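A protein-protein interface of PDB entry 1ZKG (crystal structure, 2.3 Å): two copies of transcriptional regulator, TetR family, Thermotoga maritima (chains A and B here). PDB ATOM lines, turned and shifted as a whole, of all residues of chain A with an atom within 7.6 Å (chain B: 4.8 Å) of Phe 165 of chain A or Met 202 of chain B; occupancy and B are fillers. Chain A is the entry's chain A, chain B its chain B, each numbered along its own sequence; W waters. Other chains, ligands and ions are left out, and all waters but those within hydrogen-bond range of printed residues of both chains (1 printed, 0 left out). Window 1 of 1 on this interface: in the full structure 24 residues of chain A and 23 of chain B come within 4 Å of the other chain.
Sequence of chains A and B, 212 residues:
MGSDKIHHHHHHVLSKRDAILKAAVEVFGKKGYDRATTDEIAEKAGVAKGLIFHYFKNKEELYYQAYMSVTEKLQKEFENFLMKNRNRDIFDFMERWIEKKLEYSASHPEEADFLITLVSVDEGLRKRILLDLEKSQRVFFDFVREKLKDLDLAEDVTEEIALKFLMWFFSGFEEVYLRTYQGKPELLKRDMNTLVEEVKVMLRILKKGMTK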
ATOM      1  N   PHE A 141      -1.041  -1.955   6.296  1.00  0.00           N
ATOM      2  CA  PHE A 141      -2.226  -1.786   5.477  1.00  0.00           C
ATOM      3  C   PHE A 141      -2.295  -0.514   4.685  1.00  0.00           C
ATOM      4  O   PHE A 141      -3.045  -0.458   3.688  1.00  0.00           O
ATOM      5  CB  PHE A 141      -3.504  -1.994   6.271  1.00  0.00           C
ATOM      6  CG  PHE A 141      -3.860  -3.462   6.446  1.00  0.00           C
ATOM      7  CD1 PHE A 141      -4.369  -4.196   5.382  1.00  0.00           C
ATOM      8  CD2 PHE A 141      -3.661  -4.102   7.678  1.00  0.00           C
ATOM      9  CE1 PHE A 141      -4.684  -5.522   5.529  1.00  0.00           C
ATOM     10  CE2 PHE A 141      -3.978  -5.430   7.827  1.00  0.00           C
ATOM     11  CZ  PHE A 141      -4.508  -6.132   6.750  1.00  0.00           C
ATOM     12  N   ASP A 156     -15.505  -5.782 -11.087  1.00  0.00           N
ATOM     13  CA  ASP A 156     -16.295  -5.789  -9.874  1.00  0.00           C
ATOM     14  C   ASP A 156     -15.436  -5.746  -8.613  1.00  0.00           C
ATOM     15  O   ASP A 156     -15.931  -5.399  -7.538  1.00  0.00           O
ATOM     16  CB  ASP A 156     -17.285  -6.962  -9.885  1.00  0.00           C
ATOM     17  CG  ASP A 156     -18.297  -6.867 -11.046  1.00  0.00           C
ATOM     18  OD1 ASP A 156     -18.937  -5.801 -11.203  1.00  0.00           O
ATOM     19  OD2 ASP A 156     -18.463  -7.851 -11.802  1.00  0.00           O
ATOM     20  N   VAL A 157     -14.138  -6.027  -8.741  1.00  0.00           N
ATOM     21  CA  VAL A 157     -13.231  -5.891  -7.624  1.00  0.00           C
ATOM     22  C   VAL A 157     -12.832  -4.456  -7.475  1.00  0.00           C
ATOM     23  O   VAL A 157     -11.924  -3.985  -8.167  1.00  0.00           O
ATOM     24  CB  VAL A 157     -11.938  -6.767  -7.757  1.00  0.00           C
ATOM     25  CG1 VAL A 157     -11.044  -6.590  -6.508  1.00  0.00           C
ATOM     26  CG2 VAL A 157     -12.291  -8.233  -7.931  1.00  0.00           C
ATOM     27  N   GLU A 159     -11.203  -1.323  -5.120  1.00  0.00           N
ATOM     28  CA  GLU A 159     -10.012  -1.302  -4.263  1.00  0.00           C
ATOM     29  C   GLU A 159     -10.395  -1.475  -2.803  1.00  0.00           C
ATOM     30  O   GLU A 159      -9.598  -1.981  -2.013  1.00  0.00           O
ATOM     31  CB  GLU A 159      -9.224   0.005  -4.445  1.00  0.00           C
ATOM     32  CG  GLU A 159      -8.532   0.122  -5.818  1.00  0.00           C
ATOM     33  CD  GLU A 159      -8.135   1.540  -6.182  1.00  0.00           C
ATOM     34  OE1 GLU A 159      -8.028   2.412  -5.286  1.00  0.00           O
ATOM     35  OE2 GLU A 159      -7.909   1.793  -7.381  1.00  0.00           O
ATOM     36  N   GLU A 160     -11.601  -1.007  -2.469  1.00  0.00           N
ATOM     37  CA  GLU A 160     -12.207  -1.130  -1.136  1.00  0.00           C
ATOM     38  C   GLU A 160     -12.489  -2.593  -0.780  1.00  0.00           C
ATOM     39  O   GLU A 160     -12.117  -3.041   0.291  1.00  0.00           O
ATOM     40  CB  GLU A 160     -13.518  -0.319  -1.057  1.00  0.00           C
ATOM     41  CG  GLU A 160     -14.500  -0.817   0.051  1.00  0.00           C
ATOM     42  CD  GLU A 160     -15.320   0.308   0.684  1.00  0.00           C
ATOM     43  OE1 GLU A 160     -16.057   1.014  -0.056  1.00  0.00           O
ATOM     44  OE2 GLU A 160     -15.216   0.481   1.927  1.00  0.00           O
ATOM     45  N   ILE A 161     -13.164  -3.293  -1.689  1.00  0.00           N
ATOM     46  CA  ILE A 161     -13.391  -4.743  -1.620  1.00  0.00           C
ATOM     47  C   ILE A 161     -12.085  -5.523  -1.563  1.00  0.00           C
ATOM     48  O   ILE A 161     -11.967  -6.466  -0.810  1.00  0.00           O
ATOM     49  CB  ILE A 161     -14.220  -5.215  -2.836  1.00  0.00           C
ATOM     50  CG1 ILE A 161     -15.670  -4.725  -2.688  1.00  0.00           C
ATOM     51  CG2 ILE A 161     -14.205  -6.734  -2.955  1.00  0.00           C
ATOM     52  CD1 ILE A 161     -16.553  -5.024  -3.887  1.00  0.00           C
ATOM     53  N   ALA A 162     -11.089  -5.100  -2.334  1.00  0.00           N
ATOM     54  CA  ALA A 162      -9.769  -5.747  -2.335  1.00  0.00           C
ATOM     55  C   ALA A 162      -9.138  -5.702  -0.956  1.00  0.00           C
ATOM     56  O   ALA A 162      -8.661  -6.730  -0.407  1.00  0.00           O
ATOM     57  CB  ALA A 162      -8.826  -5.075  -3.391  1.00  0.00           C
ATOM     58  N   LEU A 163      -9.147  -4.512  -0.376  1.00  0.00           N
ATOM     59  CA  LEU A 163      -8.506  -4.313   0.928  1.00  0.00           C
ATOM     60  C   LEU A 163      -9.242  -5.012   2.089  1.00  0.00           C
ATOM     61  O   LEU A 163      -8.614  -5.626   2.947  1.00  0.00           O
ATOM     62  CB  LEU A 163      -8.391  -2.812   1.162  1.00  0.00           C
ATOM     63  CG  LEU A 163      -7.577  -2.302   2.338  1.00  0.00           C
ATOM     64  CD1 LEU A 163      -6.140  -2.822   2.306  1.00  0.00           C
ATOM     65  CD2 LEU A 163      -7.633  -0.786   2.306  1.00  0.00           C
ATOM     66  N   LYS A 164     -10.572  -4.882   2.113  1.00  0.00           N
ATOM     67  CA  LYS A 164     -11.431  -5.557   3.095  1.00  0.00           C
ATOM     68  C   LYS A 164     -11.219  -7.064   3.011  1.00  0.00           C
ATOM     69  O   LYS A 164     -11.188  -7.734   4.005  1.00  0.00           O
ATOM     70  CB  LYS A 164     -12.897  -5.246   2.830  1.00  0.00           C
ATOM     71  CG  LYS A 164     -13.364  -3.944   3.398  1.00  0.00           C
ATOM     72  CD  LYS A 164     -14.822  -3.682   3.026  1.00  0.00           C
ATOM     73  CE  LYS A 164     -15.342  -2.388   3.668  1.00  0.00           C
ATOM     74  NZ  LYS A 164     -16.629  -1.888   3.075  1.00  0.00           N
ATOM     75  N   PHE A 165     -11.031  -7.587   1.813  1.00  0.00           N
ATOM     76  CA  PHE A 165     -10.890  -9.017   1.647  1.00  0.00           C
ATOM     77  C   PHE A 165      -9.593  -9.458   2.263  1.00  0.00           C
ATOM     78  O   PHE A 165      -9.569 -10.389   3.053  1.00  0.00           O
ATOM     79  CB  PHE A 165     -10.933  -9.375   0.165  1.00  0.00           C
ATOM     80  CG  PHE A 165     -10.896 -10.847  -0.117  1.00  0.00           C
ATOM     81  CD1 PHE A 165     -11.548 -11.752   0.693  1.00  0.00           C
ATOM     82  CD2 PHE A 165     -10.235 -11.317  -1.222  1.00  0.00           C
ATOM     83  CE1 PHE A 165     -11.518 -13.095   0.432  1.00  0.00           C
ATOM     84  CE2 PHE A 165     -10.220 -12.673  -1.507  1.00  0.00           C
ATOM     85  CZ  PHE A 165     -10.877 -13.560  -0.675  1.00  0.00           C
ATOM     86  N   LEU A 166      -8.508  -8.768   1.925  1.00  0.00           N
ATOM     87  CA  LEU A 166      -7.212  -9.095   2.491  1.00  0.00           C
ATOM     88  C   LEU A 166      -7.247  -8.972   4.034  1.00  0.00           C
ATOM     89  O   LEU A 166      -6.689  -9.815   4.732  1.00  0.00           O
ATOM     90  CB  LEU A 166      -6.132  -8.202   1.888  1.00  0.00           C
ATOM     91  CG  LEU A 166      -5.773  -8.499   0.440  1.00  0.00           C
ATOM     92  CD1 LEU A 166      -4.910  -7.384  -0.140  1.00  0.00           C
ATOM     93  CD2 LEU A 166      -5.079  -9.837   0.339  1.00  0.00           C
ATOM     94  N   MET A 167      -7.916  -7.940   4.551  1.00  0.00           N
ATOM     95  CA  MET A 167      -8.015  -7.741   5.998  1.00  0.00           C
ATOM     96  C   MET A 167      -8.757  -8.866   6.631  1.00  0.00           C
ATOM     97  O   MET A 167      -8.317  -9.388   7.621  1.00  0.00           O
ATOM     98  CB  MET A 167      -8.710  -6.431   6.349  1.00  0.00           C
ATOM     99  CG  MET A 167      -7.762  -5.236   6.386  1.00  0.00           C
ATOM    100  SD  MET A 167      -8.650  -3.438   6.339  1.00  0.00           S
ATOM    101  CE  MET A 167      -7.285  -2.469   7.483  1.00  0.00           C
ATOM    102  N   TRP A 168      -9.911  -9.227   6.074  1.00  0.00           N
ATOM    103  CA  TRP A 168     -10.728 -10.278   6.670  1.00  0.00           C
ATOM    104  C   TRP A 168     -10.028 -11.621   6.617  1.00  0.00           C
ATOM    105  O   TRP A 168     -10.041 -12.361   7.618  1.00  0.00           O
ATOM    106  CB  TRP A 168     -12.117 -10.379   6.046  1.00  0.00           C
ATOM    107  CG  TRP A 168     -12.872  -9.123   6.084  1.00  0.00           C
ATOM    108  CD1 TRP A 168     -12.491  -7.939   6.675  1.00  0.00           C
ATOM    109  CD2 TRP A 168     -14.133  -8.883   5.483  1.00  0.00           C
ATOM    110  NE1 TRP A 168     -13.446  -6.990   6.483  1.00  0.00           N
ATOM    111  CE2 TRP A 168     -14.469  -7.530   5.754  1.00  0.00           C
ATOM    112  CE3 TRP A 168     -15.030  -9.679   4.752  1.00  0.00           C
ATOM    113  CZ2 TRP A 168     -15.674  -6.954   5.326  1.00  0.00           C
ATOM    114  CZ3 TRP A 168     -16.224  -9.106   4.318  1.00  0.00           C
ATOM    115  CH2 TRP A 168     -16.534  -7.752   4.609  1.00  0.00           C
ATOM    116  N   PHE A 169      -9.393 -11.924   5.488  1.00  0.00           N
ATOM    117  CA  PHE A 169      -8.642 -13.176   5.361  1.00  0.00           C
ATOM    118  C   PHE A 169      -7.446 -13.278   6.330  1.00  0.00           C
ATOM    119  O   PHE A 169      -7.279 -14.310   7.002  1.00  0.00           O
ATOM    120  CB  PHE A 169      -8.212 -13.459   3.908  1.00  0.00           C
ATOM    121  CG  PHE A 169      -7.156 -14.556   3.803  1.00  0.00           C
ATOM    122  CD1 PHE A 169      -7.485 -15.893   4.082  1.00  0.00           C
ATOM    123  CD2 PHE A 169      -5.827 -14.257   3.503  1.00  0.00           C
ATOM    124  CE1 PHE A 169      -6.505 -16.905   4.020  1.00  0.00           C
ATOM    125  CE2 PHE A 169      -4.837 -15.283   3.441  1.00  0.00           C
ATOM    126  CZ  PHE A 169      -5.176 -16.579   3.697  1.00  0.00           C
ATOM    127  N   PHE A 170      -6.639 -12.219   6.445  1.00  0.00           N
ATOM    128  CA  PHE A 170      -5.517 -12.237   7.388  1.00  0.00           C
ATOM    129  C   PHE A 170      -5.944 -12.285   8.846  1.00  0.00           C
ATOM    130  O   PHE A 170      -5.279 -12.927   9.669  1.00  0.00           O
ATOM    131  CB  PHE A 170      -4.600 -11.034   7.190  1.00  0.00           C
ATOM    132  CG  PHE A 170      -3.899 -10.995   5.853  1.00  0.00           C
ATOM    133  CD1 PHE A 170      -3.704 -12.144   5.096  1.00  0.00           C
ATOM    134  CD2 PHE A 170      -3.406  -9.781   5.372  1.00  0.00           C
ATOM    135  CE1 PHE A 170      -3.055 -12.080   3.866  1.00  0.00           C
ATOM    136  CE2 PHE A 170      -2.755  -9.705   4.169  1.00  0.00           C
ATOM    137  CZ  PHE A 170      -2.578 -10.852   3.401  1.00  0.00           C
ATOM    138  N   SER A 171      -7.045 -11.620   9.190  1.00  0.00           N
ATOM    139  CA  SER A 171      -7.583 -11.719  10.555  1.00  0.00           C
ATOM    140  C   SER A 171      -8.002 -13.116  10.908  1.00  0.00           C
ATOM    141  O   SER A 171      -7.858 -13.547  12.045  1.00  0.00           O
ATOM    142  CB  SER A 171      -8.830 -10.853  10.713  1.00  0.00           C
ATOM    143  OG  SER A 171      -8.479  -9.534  10.448  1.00  0.00           O
ATOM    144  N   ILE A 205      -3.510 -17.808  -5.276  1.00  0.00           N
ATOM    145  CA  ILE A 205      -4.947 -17.792  -5.452  1.00  0.00           C
ATOM    146  C   ILE A 205      -5.471 -16.370  -5.429  1.00  0.00           C
ATOM    147  O   ILE A 205      -6.322 -15.998  -6.231  1.00  0.00           O
ATOM    148  CB  ILE A 205      -5.634 -18.623  -4.331  1.00  0.00           C
ATOM    149  CG1 ILE A 205      -5.415 -20.124  -4.567  1.00  0.00           C
ATOM    150  CG2 ILE A 205      -7.111 -18.319  -4.188  1.00  0.00           C
ATOM    151  CD1 ILE A 205      -5.888 -21.035  -3.344  1.00  0.00           C
ATOM    152  N   LEU A 206      -4.993 -15.574  -4.484  1.00  0.00           N
ATOM    153  CA  LEU A 206      -5.442 -14.186  -4.369  1.00  0.00           C
ATOM    154  C   LEU A 206      -5.044 -13.342  -5.571  1.00  0.00           C
ATOM    155  O   LEU A 206      -5.880 -12.645  -6.115  1.00  0.00           O
ATOM    156  CB  LEU A 206      -4.932 -13.558  -3.081  1.00  0.00           C
ATOM    157  CG  LEU A 206      -5.670 -14.075  -1.849  1.00  0.00           C
ATOM    158  CD1 LEU A 206      -4.944 -13.636  -0.591  1.00  0.00           C
ATOM    159  CD2 LEU A 206      -7.075 -13.605  -1.838  1.00  0.00           C
ATOM    160  N   GLY A 209      -7.175 -14.569  -8.524  1.00  0.00           N
ATOM    161  CA  GLY A 209      -8.579 -14.201  -8.383  1.00  0.00           C
ATOM    162  C   GLY A 209      -8.843 -12.700  -8.408  1.00  0.00           C
ATOM    163  O   GLY A 209      -9.930 -12.262  -8.764  1.00  0.00           O
ATOM    164  N   MET A 210      -7.851 -11.909  -8.030  1.00  0.00           N
ATOM    165  CA  MET A 210      -8.060 -10.472  -7.812  1.00  0.00           C
ATOM    166  C   MET A 210      -7.716  -9.568  -8.992  1.00  0.00           C
ATOM    167  O   MET A 210      -8.291  -8.484  -9.090  1.00  0.00           O
ATOM    168  CB  MET A 210      -7.251  -9.998  -6.607  1.00  0.00           C
ATOM    169  CG  MET A 210      -7.842 -10.414  -5.315  1.00  0.00           C
ATOM    170  SD  MET A 210      -7.083  -9.476  -3.779  1.00  0.00           S
ATOM    171  CE  MET A 210      -7.134  -7.749  -4.469  1.00  0.00           C
ATOM    172  N   PHE B 169     -11.045 -17.390   5.936  1.00  0.00           N
ATOM    173  CA  PHE B 169     -11.885 -16.341   5.466  1.00  0.00           C
ATOM    174  C   PHE B 169     -13.190 -16.211   6.239  1.00  0.00           C
ATOM    175  O   PHE B 169     -13.527 -15.101   6.677  1.00  0.00           O
ATOM    176  CB  PHE B 169     -12.207 -16.534   3.992  1.00  0.00           C
ATOM    177  CG  PHE B 169     -13.212 -15.541   3.473  1.00  0.00           C
ATOM    178  CD1 PHE B 169     -12.972 -14.164   3.579  1.00  0.00           C
ATOM    179  CD2 PHE B 169     -14.409 -15.964   2.894  1.00  0.00           C
ATOM    180  CE1 PHE B 169     -13.915 -13.234   3.113  1.00  0.00           C
ATOM    181  CE2 PHE B 169     -15.347 -15.030   2.432  1.00  0.00           C
ATOM    182  CZ  PHE B 169     -15.096 -13.675   2.539  1.00  0.00           C
ATOM    183  N   GLU B 198     -20.138  -7.160  -1.548  1.00  0.00           N
ATOM    184  CA  GLU B 198     -18.743  -7.445  -1.153  1.00  0.00           C
ATOM    185  C   GLU B 198     -18.455  -8.935  -1.136  1.00  0.00           C
ATOM    186  O   GLU B 198     -17.426  -9.393  -1.639  1.00  0.00           O
ATOM    187  CB  GLU B 198     -18.469  -6.919   0.265  1.00  0.00           C
ATOM    188  CG  GLU B 198     -18.070  -5.485   0.292  1.00  0.00           C
ATOM    189  CD  GLU B 198     -18.021  -4.896   1.683  1.00  0.00           C
ATOM    190  OE1 GLU B 198     -18.479  -5.538   2.654  1.00  0.00           O
ATOM    191  OE2 GLU B 198     -17.536  -3.746   1.788  1.00  0.00           O
ATOM    192  N   VAL B 199     -19.374  -9.668  -0.514  1.00  0.00           N
ATOM    193  CA  VAL B 199     -19.275 -11.106  -0.326  1.00  0.00           C
ATOM    194  C   VAL B 199     -19.412 -11.871  -1.640  1.00  0.00           C
ATOM    195  O   VAL B 199     -18.625 -12.774  -1.899  1.00  0.00           O
ATOM    196  CB  VAL B 199     -20.302 -11.579   0.719  1.00  0.00           C
ATOM    197  CG1 VAL B 199     -20.394 -13.126   0.767  1.00  0.00           C
ATOM    198  CG2 VAL B 199     -19.919 -11.033   2.085  1.00  0.00           C
ATOM    199  N   LYS B 200     -20.390 -11.534  -2.459  1.00  0.00           N
ATOM    200  CA  LYS B 200     -20.444 -12.068  -3.814  1.00  0.00           C
ATOM    201  C   LYS B 200     -19.090 -11.952  -4.538  1.00  0.00           C
ATOM    202  O   LYS B 200     -18.586 -12.938  -5.089  1.00  0.00           O
ATOM    203  CB  LYS B 200     -21.480 -11.310  -4.655  1.00  0.00           C
ATOM    204  CG  LYS B 200     -22.900 -11.723  -4.444  1.00  0.00           C
ATOM    205  CD  LYS B 200     -23.902 -10.766  -5.127  1.00  0.00           C
ATOM    206  CE  LYS B 200     -25.360 -11.105  -4.653  1.00  0.00           C
ATOM    207  NZ  LYS B 200     -26.416 -10.122  -5.009  1.00  0.00           N
ATOM    208  N   VAL B 201     -18.525 -10.747  -4.554  1.00  0.00           N
ATOM    209  CA  VAL B 201     -17.242 -10.503  -5.226  1.00  0.00           C
ATOM    210  C   VAL B 201     -16.074 -11.288  -4.624  1.00  0.00           C
ATOM    211  O   VAL B 201     -15.255 -11.798  -5.350  1.00  0.00           O
ATOM    212  CB  VAL B 201     -16.909  -8.980  -5.248  1.00  0.00           C
ATOM    213  CG1 VAL B 201     -15.476  -8.697  -5.739  1.00  0.00           C
ATOM    214  CG2 VAL B 201     -17.938  -8.210  -6.097  1.00  0.00           C
ATOM    215  N   MET B 202     -16.006 -11.415  -3.307  1.00  0.00           N
ATOM    216  CA  MET B 202     -14.898 -12.091  -2.655  1.00  0.00           C
ATOM    217  C   MET B 202     -14.889 -13.578  -2.955  1.00  0.00           C
ATOM    218  O   MET B 202     -13.844 -14.191  -3.097  1.00  0.00           O
ATOM    219  CB  MET B 202     -14.957 -11.867  -1.141  1.00  0.00           C
ATOM    220  CG  MET B 202     -14.654 -10.453  -0.772  1.00  0.00           C
ATOM    221  SD  MET B 202     -14.894  -9.983   1.125  1.00  0.00           S
ATOM    222  CE  MET B 202     -14.777  -7.917   1.069  1.00  0.00           C
ATOM    223  N   LEU B 203     -16.064 -14.152  -3.048  1.00  0.00           N
ATOM    224  CA  LEU B 203     -16.216 -15.563  -3.353  1.00  0.00           C
ATOM    225  C   LEU B 203     -15.958 -15.863  -4.827  1.00  0.00           C
ATOM    226  O   LEU B 203     -15.474 -16.944  -5.174  1.00  0.00           O
ATOM    227  CB  LEU B 203     -17.617 -16.036  -2.933  1.00  0.00           C
ATOM    228  CG  LEU B 203     -17.712 -16.278  -1.410  1.00  0.00           C
ATOM    229  CD1 LEU B 203     -19.142 -16.288  -0.935  1.00  0.00           C
ATOM    230  CD2 LEU B 203     -17.050 -17.576  -1.022  1.00  0.00           C
ATOM    231  N   ARG B 204     -16.321 -14.909  -5.682  1.00  0.00           N
ATOM    232  CA  ARG B 204     -15.881 -14.874  -7.076  1.00  0.00           C
ATOM    233  C   ARG B 204     -14.344 -14.834  -7.221  1.00  0.00           C
ATOM    234  O   ARG B 204     -13.763 -15.519  -8.059  1.00  0.00           O
ATOM    235  CB  ARG B 204     -16.473 -13.652  -7.764  1.00  0.00           C
ATOM    236  CG  ARG B 204     -17.736 -13.924  -8.551  1.00  0.00           C
ATOM    237  CD  ARG B 204     -17.936 -12.868  -9.670  1.00  0.00           C
ATOM    238  NE  ARG B 204     -18.879 -11.833  -9.255  1.00  0.00           N
ATOM    239  CZ  ARG B 204     -18.918 -10.598  -9.741  1.00  0.00           C
ATOM    240  NH1 ARG B 204     -18.056 -10.219 -10.684  1.00  0.00           N
ATOM    241  NH2 ARG B 204     -19.822  -9.738  -9.272  1.00  0.00           N
ATOM    242  N   ILE B 205     -13.696 -13.999  -6.422  1.00  0.00           N
ATOM    243  CA  ILE B 205     -12.244 -14.005  -6.364  1.00  0.00           C
ATOM    244  C   ILE B 205     -11.714 -15.406  -6.016  1.00  0.00           C
ATOM    245  O   ILE B 205     -10.758 -15.877  -6.624  1.00  0.00           O
ATOM    246  CB  ILE B 205     -11.749 -12.952  -5.369  1.00  0.00           C
ATOM    247  CG1 ILE B 205     -11.971 -11.538  -5.929  1.00  0.00           C
ATOM    248  CG2 ILE B 205     -10.258 -13.142  -5.006  1.00  0.00           C
ATOM    249  CD1 ILE B 205     -11.907 -10.439  -4.820  1.00  0.00           C
ATOM    250  N   LEU B 206     -12.336 -16.072  -5.040  1.00  0.00           N
ATOM    251  CA  LEU B 206     -11.825 -17.349  -4.560  1.00  0.00           C
ATOM    252  C   LEU B 206     -12.055 -18.389  -5.614  1.00  0.00           C
ATOM    253  O   LEU B 206     -11.202 -19.241  -5.824  1.00  0.00           O
ATOM    254  CB  LEU B 206     -12.448 -17.769  -3.222  1.00  0.00           C
ATOM    255  CG  LEU B 206     -11.945 -17.003  -2.004  1.00  0.00           C
ATOM    256  CD1 LEU B 206     -12.711 -17.358  -0.729  1.00  0.00           C
ATOM    257  CD2 LEU B 206     -10.437 -17.160  -1.803  1.00  0.00           C
HETATM  258  O   HOH W   1     -18.473  -3.737   4.510  1.00  0.00           O
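The side-chain carboxylate of Glu 198 of chain B is in salt-bridge range of the side-chain amino group of Lys 164 of chain A (2.4 Å).
OD2 of Asp 156 of chain A lies within salt-bridge range of NH1 of Arg 204 of chain B, 2.7 Å away.
NZ of Lys 164 of chain A lies within salt-bridge range of OE2 of Glu 160 of chain A (3.0 Å).
O of Lys 164 of chain A sits close to NE1 of Trp 168 of chain A (3.4 Å).
Among the printed residues, pairs that only touch across the chains: Asp 156 of chain A with Val 201 of chain B (3.7 Å), Val 157 of chain A with Val 201 of chain B (3.9 Å), Val 157 of chain A with Ile 205 of chain B (3.8 Å), Ile 161 of chain A with Glu 198 of chain B (3.9 Å), Ile 161 of chain A with Val 201 of chain B (3.6 Å), Ile 161 of chain A with Met 202 of chain B (3.7 Å), Lys 164 of chain A with Met 202 of chain B (3.7 Å), Phe 165 of chain A with Phe 169 of chain B (3.6 Å), Phe 165 of chain A with Met 202 of chain B (3.7 Å), Phe 165 of chain A with Ile 205 of chain B (3.5 Å), Phe 165 of chain A with Leu 206 of chain B (3.8 Å), Trp 168 of chain A with Glu 198 of chain B (3.5 Å), Trp 168 of chain A with Met 202 of chain B (3.6 Å), Gly 209 of chain A with Ile 205 of chain B (3.3 Å) and Met 210 of chain A with Ile 205 of chain B (3.7 Å).
Of the printed residues of chain B, Phe 165 of chain A touches Phe 169, Met 202, Ile 205 and Leu 206.
Met 202 of chain B touches four residues of chain A.
Printed residues of chain B within 4 Å of Asp 156 of chain A: Val 201 (3.7 Å) and Arg 204 (2.7 Å).
Printed residues of chain B within 4 Å of Ile 161 of chain A: Glu 198, Val 201 and Met 202.
Of the printed residues of chain A, Phe 169 of chain B touches Phe 165 (3.6 Å).
Of the printed residues of chain A, Glu 198 of chain B touches Ile 161, Lys 164 and Trp 168.
Hydrophobic or aromatic side chains of chain A that line the printed part of chain B: Val 157, Ile 161, Phe 165, Trp 168 and Met 210.
Of the 10 printed residues of chain B, 7 touch a printed residue of chain A.
Hydrophobic or aromatic side chains of chain B within 4 Å of the printed part of chain A: Phe 169, Val 201, Met 202, Ile 205 and Leu 206.
Along chain B the printed residues that touch a printed residue of chain A span positions 169 to 206.
Among the printed residues, Asp or Glu carboxylates within 4 Å of a Lys or Arg side-chain nitrogen of the other chain: Asp 156 of chain A with Arg 204 of chain B (2.7 Å) and Lys 164 of chain A with Glu 198 of chain B (2.4 Å).
Positions printed for both chains: 169, 205 and 206.
Of the 17 pairs that touch across the chains among the printed residues, none has its exchanged pair printed and touching as well.
Water W1 bridges the side-chain carboxylate (OE1) of Glu 198 of chain B and the side-chain amino group (NZ) of Lys 164 of chain A.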
